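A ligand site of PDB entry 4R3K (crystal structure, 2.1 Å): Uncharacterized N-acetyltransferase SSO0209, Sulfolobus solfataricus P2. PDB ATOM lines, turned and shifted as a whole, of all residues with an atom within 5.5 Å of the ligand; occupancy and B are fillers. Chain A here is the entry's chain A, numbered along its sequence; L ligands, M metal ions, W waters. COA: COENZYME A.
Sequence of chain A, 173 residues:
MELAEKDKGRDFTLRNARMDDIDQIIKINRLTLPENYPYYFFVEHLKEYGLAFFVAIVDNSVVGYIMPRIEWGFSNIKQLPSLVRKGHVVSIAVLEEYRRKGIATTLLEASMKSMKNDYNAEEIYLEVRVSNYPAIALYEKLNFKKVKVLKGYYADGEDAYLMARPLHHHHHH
The backbone carbonyl oxygen of Val 94 is in hydrogen-bond range of the guanidinium group of Arg 99, at 2.8 Å. O of Gly 102 is in hydrogen-bond range of OG1 of Thr 106, 3.2 Å away. The backbone NH (N) of Ala 135 sits at hydrogen-bond distance from the side-chain amide oxygen (OD1) of Asn 132 (3.4 Å). The side-chain hydroxyl (OG1) of Thr 106 sits at hydrogen-bond distance from the backbone carbonyl oxygen (O) of Ile 103.
O9P of the ligand lies within hydrogen-bond range of N of Val 94, 2.6 Å away. The backbone NH (N) of Thr 105 sits at hydrogen-bond distance from an oxygen (O2A) of the ligand (3.0 Å). OG1 of Thr 105 lies within hydrogen-bond range of O2A of the ligand. An oxygen (O4A) of the ligand lies within hydrogen-bond range of the backbone NH (N) of Arg 100, 2.8 Å away. The guanidinium group (NH2) of Arg 100 is in salt-bridge range of an oxygen (O9A) of the ligand (3.0 Å). O of Ile 92 sits at hydrogen-bond distance from N4P of the ligand, at 2.8 Å. N of Gly 102 lies within hydrogen-bond range of O1A of the ligand, 2.8 Å away. ND2 of Asn 132 is in hydrogen-bond range of O5P of the ligand, at 2.9 Å. The side-chain hydroxyl of Tyr 139 lies close to a sulfur (S1P) of the ligand (3.0 Å). N of Ala 104 is in hydrogen-bond range of O5A of the ligand (3.1 Å). The backbone NH (N) of Lys 101 lies within hydrogen-bond range of an oxygen (O1A) of the ligand, 3.2 Å away. S1P of the ligand sits close to O of Glu 127 (3.6 Å).
Residues that only touch the ligand: Arg 99 (3.2 Å), Leu 138 (3.3 Å), Tyr 133 (3.4 Å), Ala 93 (3.4 Å), Pro 134 (3.5 Å), Lys 141 (3.5 Å), Ile 103 (3.6 Å), Leu 33 (3.6 Å), Ala 137 (3.6 Å) and Ala 135 (3.96 Å). Hydrophobic or aromatic side chains within 4 Å of the ligand: Leu 33, Val 94, Ile 103, Ala 104, Tyr 133, Pro 134, Ala 137 and Leu 138. The nearest printed residue that does not touch the ligand is Thr 32 (4.03 Å).
Water W2 lies within hydrogen-bond range of N8P of the ligand and OD1 of Asn 132.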
ATOM      1  N   THR A  32      -7.114 -22.154  17.210  1.00  0.00           N
ATOM      2  CA  THR A  32      -8.557 -22.244  16.937  1.00  0.00           C
ATOM      3  C   THR A  32      -9.308 -20.946  17.191  1.00  0.00           C
ATOM      4  O   THR A  32     -10.417 -20.770  16.692  1.00  0.00           O
ATOM      5  CB  THR A  32      -9.207 -23.354  17.793  1.00  0.00           C
ATOM      6  OG1 THR A  32      -9.035 -23.034  19.177  1.00  0.00           O
ATOM      7  CG2 THR A  32      -8.583 -24.705  17.517  1.00  0.00           C
ATOM      8  N   LEU A  33      -8.726 -20.049  17.978  1.00  0.00           N
ATOM      9  CA  LEU A  33      -9.416 -18.826  18.373  1.00  0.00           C
ATOM     10  C   LEU A  33      -8.554 -17.588  18.127  1.00  0.00           C
ATOM     11  O   LEU A  33      -7.323 -17.660  18.147  1.00  0.00           O
ATOM     12  CB  LEU A  33      -9.819 -18.907  19.839  1.00  0.00           C
ATOM     13  CG  LEU A  33     -10.868 -19.959  20.211  1.00  0.00           C
ATOM     14  CD1 LEU A  33     -11.009 -20.091  21.731  1.00  0.00           C
ATOM     15  CD2 LEU A  33     -12.197 -19.607  19.584  1.00  0.00           C
ATOM     16  N   ILE A  92     -14.012 -21.881  24.936  1.00  0.00           N
ATOM     17  CA  ILE A  92     -14.112 -23.314  24.680  1.00  0.00           C
ATOM     18  C   ILE A  92     -13.625 -23.600  23.268  1.00  0.00           C
ATOM     19  O   ILE A  92     -13.873 -22.818  22.334  1.00  0.00           O
ATOM     20  CB  ILE A  92     -15.562 -23.829  24.878  1.00  0.00           C
ATOM     21  CG1 ILE A  92     -15.664 -25.318  24.524  1.00  0.00           C
ATOM     22  CG2 ILE A  92     -16.540 -22.994  24.074  1.00  0.00           C
ATOM     23  CD1 ILE A  92     -16.965 -25.980  24.941  1.00  0.00           C
ATOM     24  N   ALA A  93     -12.901 -24.706  23.103  1.00  0.00           N
ATOM     25  CA  ALA A  93     -12.338 -25.044  21.798  1.00  0.00           C
ATOM     26  C   ALA A  93     -11.990 -26.528  21.739  1.00  0.00           C
ATOM     27  O   ALA A  93     -11.658 -27.140  22.744  1.00  0.00           O
ATOM     28  CB  ALA A  93     -11.083 -24.215  21.517  1.00  0.00           C
ATOM     29  N   VAL A  94     -12.078 -27.089  20.530  1.00  0.00           N
ATOM     30  CA  VAL A  94     -11.785 -28.496  20.301  1.00  0.00           C
ATOM     31  C   VAL A  94     -10.960 -28.600  19.028  1.00  0.00           C
ATOM     32  O   VAL A  94     -11.311 -27.993  18.008  1.00  0.00           O
ATOM     33  CB  VAL A  94     -13.091 -29.317  20.191  1.00  0.00           C
ATOM     34  CG1 VAL A  94     -12.819 -30.696  19.600  1.00  0.00           C
ATOM     35  CG2 VAL A  94     -13.757 -29.422  21.567  1.00  0.00           C
ATOM     36  N   LEU A  95      -9.837 -29.331  19.081  1.00  0.00           N
ATOM     37  CA  LEU A  95      -8.975 -29.457  17.897  1.00  0.00           C
ATOM     38  C   LEU A  95      -9.746 -29.994  16.704  1.00  0.00           C
ATOM     39  O   LEU A  95     -10.609 -30.862  16.842  1.00  0.00           O
ATOM     40  CB  LEU A  95      -7.766 -30.364  18.192  1.00  0.00           C
ATOM     41  CG  LEU A  95      -6.630 -29.780  19.048  1.00  0.00           C
ATOM     42  CD1 LEU A  95      -5.546 -30.828  19.264  1.00  0.00           C
ATOM     43  CD2 LEU A  95      -6.026 -28.517  18.428  1.00  0.00           C
ATOM     44  N   TYR A  98     -10.693 -33.640  15.981  1.00  0.00           N
ATOM     45  CA  TYR A  98     -11.498 -34.338  16.976  1.00  0.00           C
ATOM     46  C   TYR A  98     -12.905 -33.760  17.138  1.00  0.00           C
ATOM     47  O   TYR A  98     -13.596 -34.082  18.102  1.00  0.00           O
ATOM     48  CB  TYR A  98     -10.772 -34.330  18.328  1.00  0.00           C
ATOM     49  CG  TYR A  98      -9.469 -35.101  18.283  1.00  0.00           C
ATOM     50  CD1 TYR A  98      -9.462 -36.492  18.403  1.00  0.00           C
ATOM     51  CD2 TYR A  98      -8.253 -34.456  18.114  1.00  0.00           C
ATOM     52  CE1 TYR A  98      -8.271 -37.217  18.347  1.00  0.00           C
ATOM     53  CE2 TYR A  98      -7.058 -35.175  18.071  1.00  0.00           C
ATOM     54  CZ  TYR A  98      -7.077 -36.552  18.185  1.00  0.00           C
ATOM     55  OH  TYR A  98      -5.903 -37.277  18.136  1.00  0.00           O
ATOM     56  N   ARG A  99     -13.335 -32.958  16.176  1.00  0.00           N
ATOM     57  CA  ARG A  99     -14.665 -32.364  16.222  1.00  0.00           C
ATOM     58  C   ARG A  99     -15.768 -33.342  15.787  1.00  0.00           C
ATOM     59  O   ARG A  99     -15.479 -34.398  15.232  1.00  0.00           O
ATOM     60  CB  ARG A  99     -14.696 -31.095  15.360  1.00  0.00           C
ATOM     61  CG  ARG A  99     -13.822 -29.996  15.938  1.00  0.00           C
ATOM     62  CD  ARG A  99     -13.739 -28.757  15.079  1.00  0.00           C
ATOM     63  NE  ARG A  99     -12.808 -27.809  15.669  1.00  0.00           N
ATOM     64  CZ  ARG A  99     -12.247 -26.784  15.013  1.00  0.00           C
ATOM     65  NH1 ARG A  99     -12.536 -26.579  13.742  1.00  0.00           N
ATOM     66  NH2 ARG A  99     -11.403 -25.980  15.646  1.00  0.00           N
ATOM     67  N   ARG A 100     -17.017 -32.973  16.061  1.00  0.00           N
ATOM     68  CA  ARG A 100     -18.194 -33.805  15.784  1.00  0.00           C
ATOM     69  C   ARG A 100     -18.157 -35.142  16.509  1.00  0.00           C
ATOM     70  O   ARG A 100     -18.710 -36.124  16.010  1.00  0.00           O
ATOM     71  CB  ARG A 100     -18.357 -34.051  14.273  1.00  0.00           C
ATOM     72  CG  ARG A 100     -18.286 -32.811  13.401  1.00  0.00           C
ATOM     73  CD  ARG A 100     -19.152 -31.665  13.927  1.00  0.00           C
ATOM     74  NE  ARG A 100     -20.590 -31.900  13.778  1.00  0.00           N
ATOM     75  CZ  ARG A 100     -21.266 -31.706  12.658  1.00  0.00           C
ATOM     76  NH1 ARG A 100     -20.641 -31.287  11.552  1.00  0.00           N
ATOM     77  NH2 ARG A 100     -22.576 -31.929  12.620  1.00  0.00           N
ATOM     78  N   LYS A 101     -17.533 -35.198  17.689  1.00  0.00           N
ATOM     79  CA  LYS A 101     -17.491 -36.427  18.474  1.00  0.00           C
ATOM     80  C   LYS A 101     -18.215 -36.302  19.822  1.00  0.00           C
ATOM     81  O   LYS A 101     -18.212 -37.220  20.631  1.00  0.00           O
ATOM     82  CB  LYS A 101     -16.046 -36.873  18.720  1.00  0.00           C
ATOM     83  CG  LYS A 101     -15.290 -37.312  17.481  1.00  0.00           C
ATOM     84  CD  LYS A 101     -13.872 -37.758  17.813  1.00  0.00           C
ATOM     85  CE  LYS A 101     -13.815 -39.159  18.436  1.00  0.00           C
ATOM     86  NZ  LYS A 101     -14.266 -40.230  17.491  1.00  0.00           N
ATOM     87  N   GLY A 102     -18.841 -35.152  20.042  1.00  0.00           N
ATOM     88  CA  GLY A 102     -19.505 -34.886  21.300  1.00  0.00           C
ATOM     89  C   GLY A 102     -18.624 -34.250  22.371  1.00  0.00           C
ATOM     90  O   GLY A 102     -19.056 -34.100  23.507  1.00  0.00           O
ATOM     91  N   ILE A 103     -17.398 -33.869  22.021  1.00  0.00           N
ATOM     92  CA  ILE A 103     -16.465 -33.357  23.033  1.00  0.00           C
ATOM     93  C   ILE A 103     -16.917 -32.033  23.642  1.00  0.00           C
ATOM     94  O   ILE A 103     -16.917 -31.854  24.866  1.00  0.00           O
ATOM     95  CB  ILE A 103     -15.040 -33.204  22.465  1.00  0.00           C
ATOM     96  CG1 ILE A 103     -14.433 -34.584  22.193  1.00  0.00           C
ATOM     97  CG2 ILE A 103     -14.164 -32.447  23.440  1.00  0.00           C
ATOM     98  CD1 ILE A 103     -13.042 -34.511  21.571  1.00  0.00           C
ATOM     99  N   ALA A 104     -17.315 -31.091  22.789  1.00  0.00           N
ATOM    100  CA  ALA A 104     -17.737 -29.795  23.290  1.00  0.00           C
ATOM    101  C   ALA A 104     -18.997 -29.963  24.130  1.00  0.00           C
ATOM    102  O   ALA A 104     -19.102 -29.381  25.195  1.00  0.00           O
ATOM    103  CB  ALA A 104     -17.963 -28.827  22.149  1.00  0.00           C
ATOM    104  N   THR A 105     -19.924 -30.784  23.642  1.00  0.00           N
ATOM    105  CA  THR A 105     -21.140 -31.088  24.389  1.00  0.00           C
ATOM    106  C   THR A 105     -20.839 -31.608  25.784  1.00  0.00           C
ATOM    107  O   THR A 105     -21.410 -31.131  26.749  1.00  0.00           O
ATOM    108  CB  THR A 105     -22.006 -32.133  23.652  1.00  0.00           C
ATOM    109  OG1 THR A 105     -22.422 -31.592  22.388  1.00  0.00           O
ATOM    110  CG2 THR A 105     -23.232 -32.478  24.477  1.00  0.00           C
ATOM    111  N   THR A 106     -19.925 -32.568  25.897  1.00  0.00           N
ATOM    112  CA  THR A 106     -19.591 -33.124  27.205  1.00  0.00           C
ATOM    113  C   THR A 106     -18.796 -32.144  28.055  1.00  0.00           C
ATOM    114  O   THR A 106     -18.931 -32.119  29.279  1.00  0.00           O
ATOM    115  CB  THR A 106     -18.794 -34.447  27.072  1.00  0.00           C
ATOM    116  OG1 THR A 106     -17.587 -34.220  26.317  1.00  0.00           O
ATOM    117  CG2 THR A 106     -19.626 -35.523  26.371  1.00  0.00           C
ATOM    118  N   LEU A 126     -22.699 -16.964  27.729  1.00  0.00           N
ATOM    119  CA  LEU A 126     -21.471 -16.819  26.932  1.00  0.00           C
ATOM    120  C   LEU A 126     -21.712 -15.818  25.831  1.00  0.00           C
ATOM    121  O   LEU A 126     -22.856 -15.466  25.552  1.00  0.00           O
ATOM    122  CB  LEU A 126     -21.050 -18.157  26.325  1.00  0.00           C
ATOM    123  CG  LEU A 126     -22.163 -18.912  25.575  1.00  0.00           C
ATOM    124  CD1 LEU A 126     -22.374 -18.425  24.126  1.00  0.00           C
ATOM    125  CD2 LEU A 126     -21.908 -20.401  25.609  1.00  0.00           C
ATOM    126  N   GLU A 127     -20.633 -15.411  25.163  1.00  0.00           N
ATOM    127  CA  GLU A 127     -20.752 -14.658  23.928  1.00  0.00           C
ATOM    128  C   GLU A 127     -20.240 -15.508  22.749  1.00  0.00           C
ATOM    129  O   GLU A 127     -19.291 -16.294  22.893  1.00  0.00           O
ATOM    130  CB  GLU A 127     -19.988 -13.339  24.045  1.00  0.00           C
ATOM    131  CG  GLU A 127     -20.562 -12.386  25.094  1.00  0.00           C
ATOM    132  CD  GLU A 127     -19.989 -12.584  26.490  1.00  0.00           C
ATOM    133  OE1 GLU A 127     -19.049 -13.401  26.670  1.00  0.00           O
ATOM    134  OE2 GLU A 127     -20.473 -11.907  27.416  1.00  0.00           O
ATOM    135  N   VAL A 128     -20.881 -15.383  21.590  1.00  0.00           N
ATOM    136  CA  VAL A 128     -20.427 -16.097  20.398  1.00  0.00           C
ATOM    137  C   VAL A 128     -20.552 -15.168  19.184  1.00  0.00           C
ATOM    138  O   VAL A 128     -21.531 -14.434  19.071  1.00  0.00           O
ATOM    139  CB  VAL A 128     -21.261 -17.399  20.174  1.00  0.00           C
ATOM    140  CG1 VAL A 128     -22.755 -17.099  20.194  1.00  0.00           C
ATOM    141  CG2 VAL A 128     -20.880 -18.083  18.885  1.00  0.00           C
ATOM    142  N   ARG A 129     -19.554 -15.182  18.294  1.00  0.00           N
ATOM    143  CA  ARG A 129     -19.630 -14.435  17.026  1.00  0.00           C
ATOM    144  C   ARG A 129     -20.885 -14.803  16.251  1.00  0.00           C
ATOM    145  O   ARG A 129     -21.205 -15.982  16.149  1.00  0.00           O
ATOM    146  CB  ARG A 129     -18.402 -14.716  16.138  1.00  0.00           C
ATOM    147  CG  ARG A 129     -17.145 -13.972  16.529  1.00  0.00           C
ATOM    148  CD  ARG A 129     -16.002 -14.269  15.590  1.00  0.00           C
ATOM    149  NE  ARG A 129     -14.757 -13.702  16.079  1.00  0.00           N
ATOM    150  CZ  ARG A 129     -14.287 -12.500  15.733  1.00  0.00           C
ATOM    151  NH1 ARG A 129     -14.967 -11.751  14.877  1.00  0.00           N
ATOM    152  NH2 ARG A 129     -13.155 -12.061  16.250  1.00  0.00           N
ATOM    153  N   ASN A 132     -20.429 -17.486  13.792  1.00  0.00           N
ATOM    154  CA  ASN A 132     -19.924 -18.783  14.233  1.00  0.00           C
ATOM    155  C   ASN A 132     -21.017 -19.857  14.235  1.00  0.00           C
ATOM    156  O   ASN A 132     -21.409 -20.354  15.293  1.00  0.00           O
ATOM    157  CB  ASN A 132     -19.298 -18.670  15.631  1.00  0.00           C
ATOM    158  CG  ASN A 132     -18.405 -19.866  15.970  1.00  0.00           C
ATOM    159  OD1 ASN A 132     -18.457 -20.900  15.290  1.00  0.00           O
ATOM    160  ND2 ASN A 132     -17.581 -19.714  16.993  1.00  0.00           N
ATOM    161  N   TYR A 133     -21.468 -20.207  13.033  1.00  0.00           N
ATOM    162  CA  TYR A 133     -22.506 -21.202  12.826  1.00  0.00           C
ATOM    163  C   TYR A 133     -22.352 -22.500  13.651  1.00  0.00           C
ATOM    164  O   TYR A 133     -23.315 -22.942  14.280  1.00  0.00           O
ATOM    165  CB  TYR A 133     -22.593 -21.514  11.317  1.00  0.00           C
ATOM    166  CG  TYR A 133     -23.580 -22.597  10.931  1.00  0.00           C
ATOM    167  CD1 TYR A 133     -24.867 -22.274  10.506  1.00  0.00           C
ATOM    168  CD2 TYR A 133     -23.222 -23.937  10.946  1.00  0.00           C
ATOM    169  CE1 TYR A 133     -25.767 -23.260  10.135  1.00  0.00           C
ATOM    170  CE2 TYR A 133     -24.108 -24.923  10.579  1.00  0.00           C
ATOM    171  CZ  TYR A 133     -25.385 -24.588  10.177  1.00  0.00           C
ATOM    172  OH  TYR A 133     -26.276 -25.567   9.799  1.00  0.00           O
ATOM    173  N   PRO A 134     -21.143 -23.116  13.659  1.00  0.00           N
ATOM    174  CA  PRO A 134     -21.064 -24.385  14.398  1.00  0.00           C
ATOM    175  C   PRO A 134     -21.278 -24.216  15.902  1.00  0.00           C
ATOM    176  O   PRO A 134     -21.892 -25.075  16.528  1.00  0.00           O
ATOM    177  CB  PRO A 134     -19.642 -24.884  14.112  1.00  0.00           C
ATOM    178  CG  PRO A 134     -19.260 -24.207  12.827  1.00  0.00           C
ATOM    179  CD  PRO A 134     -19.896 -22.849  12.926  1.00  0.00           C
ATOM    180  N   ALA A 135     -20.754 -23.131  16.453  1.00  0.00           N
ATOM    181  CA  ALA A 135     -20.876 -22.874  17.882  1.00  0.00           C
ATOM    182  C   ALA A 135     -22.325 -22.565  18.261  1.00  0.00           C
ATOM    183  O   ALA A 135     -22.830 -23.051  19.276  1.00  0.00           O
ATOM    184  CB  ALA A 135     -19.973 -21.728  18.295  1.00  0.00           C
ATOM    185  N   ALA A 137     -25.029 -23.488  16.677  1.00  0.00           N
ATOM    186  CA  ALA A 137     -25.748 -24.751  16.562  1.00  0.00           C
ATOM    187  C   ALA A 137     -25.605 -25.585  17.839  1.00  0.00           C
ATOM    188  O   ALA A 137     -26.598 -26.097  18.364  1.00  0.00           O
ATOM    189  CB  ALA A 137     -25.268 -25.536  15.371  1.00  0.00           C
ATOM    190  N   LEU A 138     -24.374 -25.719  18.316  1.00  0.00           N
ATOM    191  CA  LEU A 138     -24.091 -26.501  19.525  1.00  0.00           C
ATOM    192  C   LEU A 138     -24.843 -25.940  20.733  1.00  0.00           C
ATOM    193  O   LEU A 138     -25.483 -26.685  21.463  1.00  0.00           O
ATOM    194  CB  LEU A 138     -22.575 -26.519  19.806  1.00  0.00           C
ATOM    195  CG  LEU A 138     -22.028 -26.627  21.233  1.00  0.00           C
ATOM    196  CD1 LEU A 138     -22.044 -28.055  21.755  1.00  0.00           C
ATOM    197  CD2 LEU A 138     -20.627 -26.063  21.335  1.00  0.00           C
ATOM    198  N   TYR A 139     -24.783 -24.622  20.921  1.00  0.00           N
ATOM    199  CA  TYR A 139     -25.392 -24.003  22.082  1.00  0.00           C
ATOM    200  C   TYR A 139     -26.910 -24.168  22.075  1.00  0.00           C
ATOM    201  O   TYR A 139     -27.527 -24.482  23.097  1.00  0.00           O
ATOM    202  CB  TYR A 139     -25.019 -22.518  22.156  1.00  0.00           C
ATOM    203  CG  TYR A 139     -23.527 -22.281  22.256  1.00  0.00           C
ATOM    204  CD1 TYR A 139     -22.693 -23.173  22.910  1.00  0.00           C
ATOM    205  CD2 TYR A 139     -22.954 -21.150  21.692  1.00  0.00           C
ATOM    206  CE1 TYR A 139     -21.314 -22.961  22.993  1.00  0.00           C
ATOM    207  CE2 TYR A 139     -21.588 -20.923  21.773  1.00  0.00           C
ATOM    208  CZ  TYR A 139     -20.775 -21.822  22.422  1.00  0.00           C
ATOM    209  OH  TYR A 139     -19.418 -21.566  22.483  1.00  0.00           O
ATOM    210  N   LYS A 141     -28.571 -26.488  20.642  1.00  0.00           N
ATOM    211  CA  LYS A 141     -28.882 -27.898  20.895  1.00  0.00           C
ATOM    212  C   LYS A 141     -28.899 -28.165  22.392  1.00  0.00           C
ATOM    213  O   LYS A 141     -29.639 -29.010  22.867  1.00  0.00           O
ATOM    214  CB  LYS A 141     -27.882 -28.806  20.189  1.00  0.00           C
ATOM    215  CG  LYS A 141     -28.383 -30.226  19.948  1.00  0.00           C
ATOM    216  CD  LYS A 141     -27.430 -31.012  19.046  1.00  0.00           C
ATOM    217  CE  LYS A 141     -27.770 -32.496  19.051  1.00  0.00           C
ATOM    218  NZ  LYS A 141     -27.866 -33.030  20.439  1.00  0.00           N
HETATM  219  N1A COA L   1     -21.849 -27.569  11.804  1.00  0.00           N
HETATM  220  C2A COA L   1     -23.166 -27.698  12.213  1.00  0.00           C
HETATM  221  N3A COA L   1     -23.461 -28.087  13.506  1.00  0.00           N
HETATM  222  C4A COA L   1     -22.443 -28.339  14.380  1.00  0.00           C
HETATM  223  C5A COA L   1     -21.114 -28.225  13.983  1.00  0.00           C
HETATM  224  C6A COA L   1     -20.817 -27.836  12.680  1.00  0.00           C
HETATM  225  N6A COA L   1     -19.560 -27.875  12.256  1.00  0.00           N
HETATM  226  N7A COA L   1     -20.327 -28.544  15.037  1.00  0.00           N
HETATM  227  C8A COA L   1     -21.138 -28.856  16.089  1.00  0.00           C
HETATM  228  N9A COA L   1     -22.437 -28.734  15.688  1.00  0.00           N
HETATM  229  C1B COA L   1     -23.651 -29.061  16.455  1.00  0.00           C
HETATM  230  C2B COA L   1     -24.120 -30.415  15.979  1.00  0.00           C
HETATM  231  O2B COA L   1     -25.518 -30.469  16.170  1.00  0.00           O
HETATM  232  C3B COA L   1     -23.477 -31.376  16.935  1.00  0.00           C
HETATM  233  O3B COA L   1     -24.231 -32.566  16.993  1.00  0.00           O
HETATM  234  P3B COA L   1     -24.068 -33.659  15.813  1.00  0.00           P
HETATM  235  O7A COA L   1     -24.808 -34.911  16.229  1.00  0.00           O
HETATM  236  O8A COA L   1     -22.602 -33.967  15.622  1.00  0.00           O
HETATM  237  O9A COA L   1     -24.638 -33.114  14.525  1.00  0.00           O
HETATM  238  C4B COA L   1     -23.485 -30.578  18.222  1.00  0.00           C
HETATM  239  O4B COA L   1     -23.317 -29.239  17.819  1.00  0.00           O
HETATM  240  C5B COA L   1     -22.378 -30.924  19.201  1.00  0.00           C
HETATM  241  O5B COA L   1     -21.178 -31.106  18.519  1.00  0.00           O
HETATM  242  P1A COA L   1     -19.868 -31.461  19.367  1.00  0.00           P
HETATM  243  O1A COA L   1     -19.188 -32.668  18.755  1.00  0.00           O
HETATM  244  O2A COA L   1     -20.220 -31.647  20.816  1.00  0.00           O
HETATM  245  O3A COA L   1     -18.975 -30.148  19.154  1.00  0.00           O
HETATM  246  P2A COA L   1     -17.414 -30.207  18.827  1.00  0.00           P
HETATM  247  O4A COA L   1     -17.146 -30.537  17.384  1.00  0.00           O
HETATM  248  O5A COA L   1     -16.737 -31.167  19.760  1.00  0.00           O
HETATM  249  O6A COA L   1     -16.902 -28.694  19.066  1.00  0.00           O
HETATM  250  CBP COA L   1     -16.814 -26.351  18.717  1.00  0.00           C
HETATM  251  CCP COA L   1     -17.716 -27.586  18.749  1.00  0.00           C
HETATM  252  CDP COA L   1     -17.665 -25.156  18.285  1.00  0.00           C
HETATM  253  CEP COA L   1     -16.228 -26.110  20.116  1.00  0.00           C
HETATM  254  CAP COA L   1     -15.675 -26.617  17.738  1.00  0.00           C
HETATM  255  OAP COA L   1     -16.143 -26.546  16.408  1.00  0.00           O
HETATM  256  C9P COA L   1     -14.560 -25.602  17.861  1.00  0.00           C
HETATM  257  O9P COA L   1     -13.474 -25.847  18.719  1.00  0.00           O
HETATM  258  N8P COA L   1     -14.656 -24.502  17.106  1.00  0.00           N
HETATM  259  C7P COA L   1     -13.590 -23.511  17.082  1.00  0.00           C
HETATM  260  C6P COA L   1     -13.472 -22.754  18.414  1.00  0.00           C
HETATM  261  C5P COA L   1     -14.750 -21.995  18.709  1.00  0.00           C
HETATM  262  O5P COA L   1     -15.385 -21.448  17.786  1.00  0.00           O
HETATM  263  N4P COA L   1     -15.135 -21.948  19.982  1.00  0.00           N
HETATM  264  C3P COA L   1     -16.405 -21.366  20.349  1.00  0.00           C
HETATM  265  C2P COA L   1     -16.339 -19.859  20.572  1.00  0.00           C
HETATM  266  S1P COA L   1     -17.741 -19.210  21.520  1.00  0.00           S
HETATM  267 CA    CA M   1     -16.911 -16.988  18.616  1.00  0.00          CA
HETATM  268  O   HOH W   1     -16.207 -33.575  19.225  1.00  0.00           O
HETATM  269  O   HOH W   2     -16.376 -23.162  15.199  1.00  0.00           O
HETATM  270  O   HOH W   3     -21.340 -34.273  17.654  1.00  0.00           O
HETATM  271  O   HOH W   4     -16.937 -28.968  12.912  1.00  0.00           O
HETATM  272  O   HOH W   5     -17.589 -28.843  15.487  1.00  0.00           O
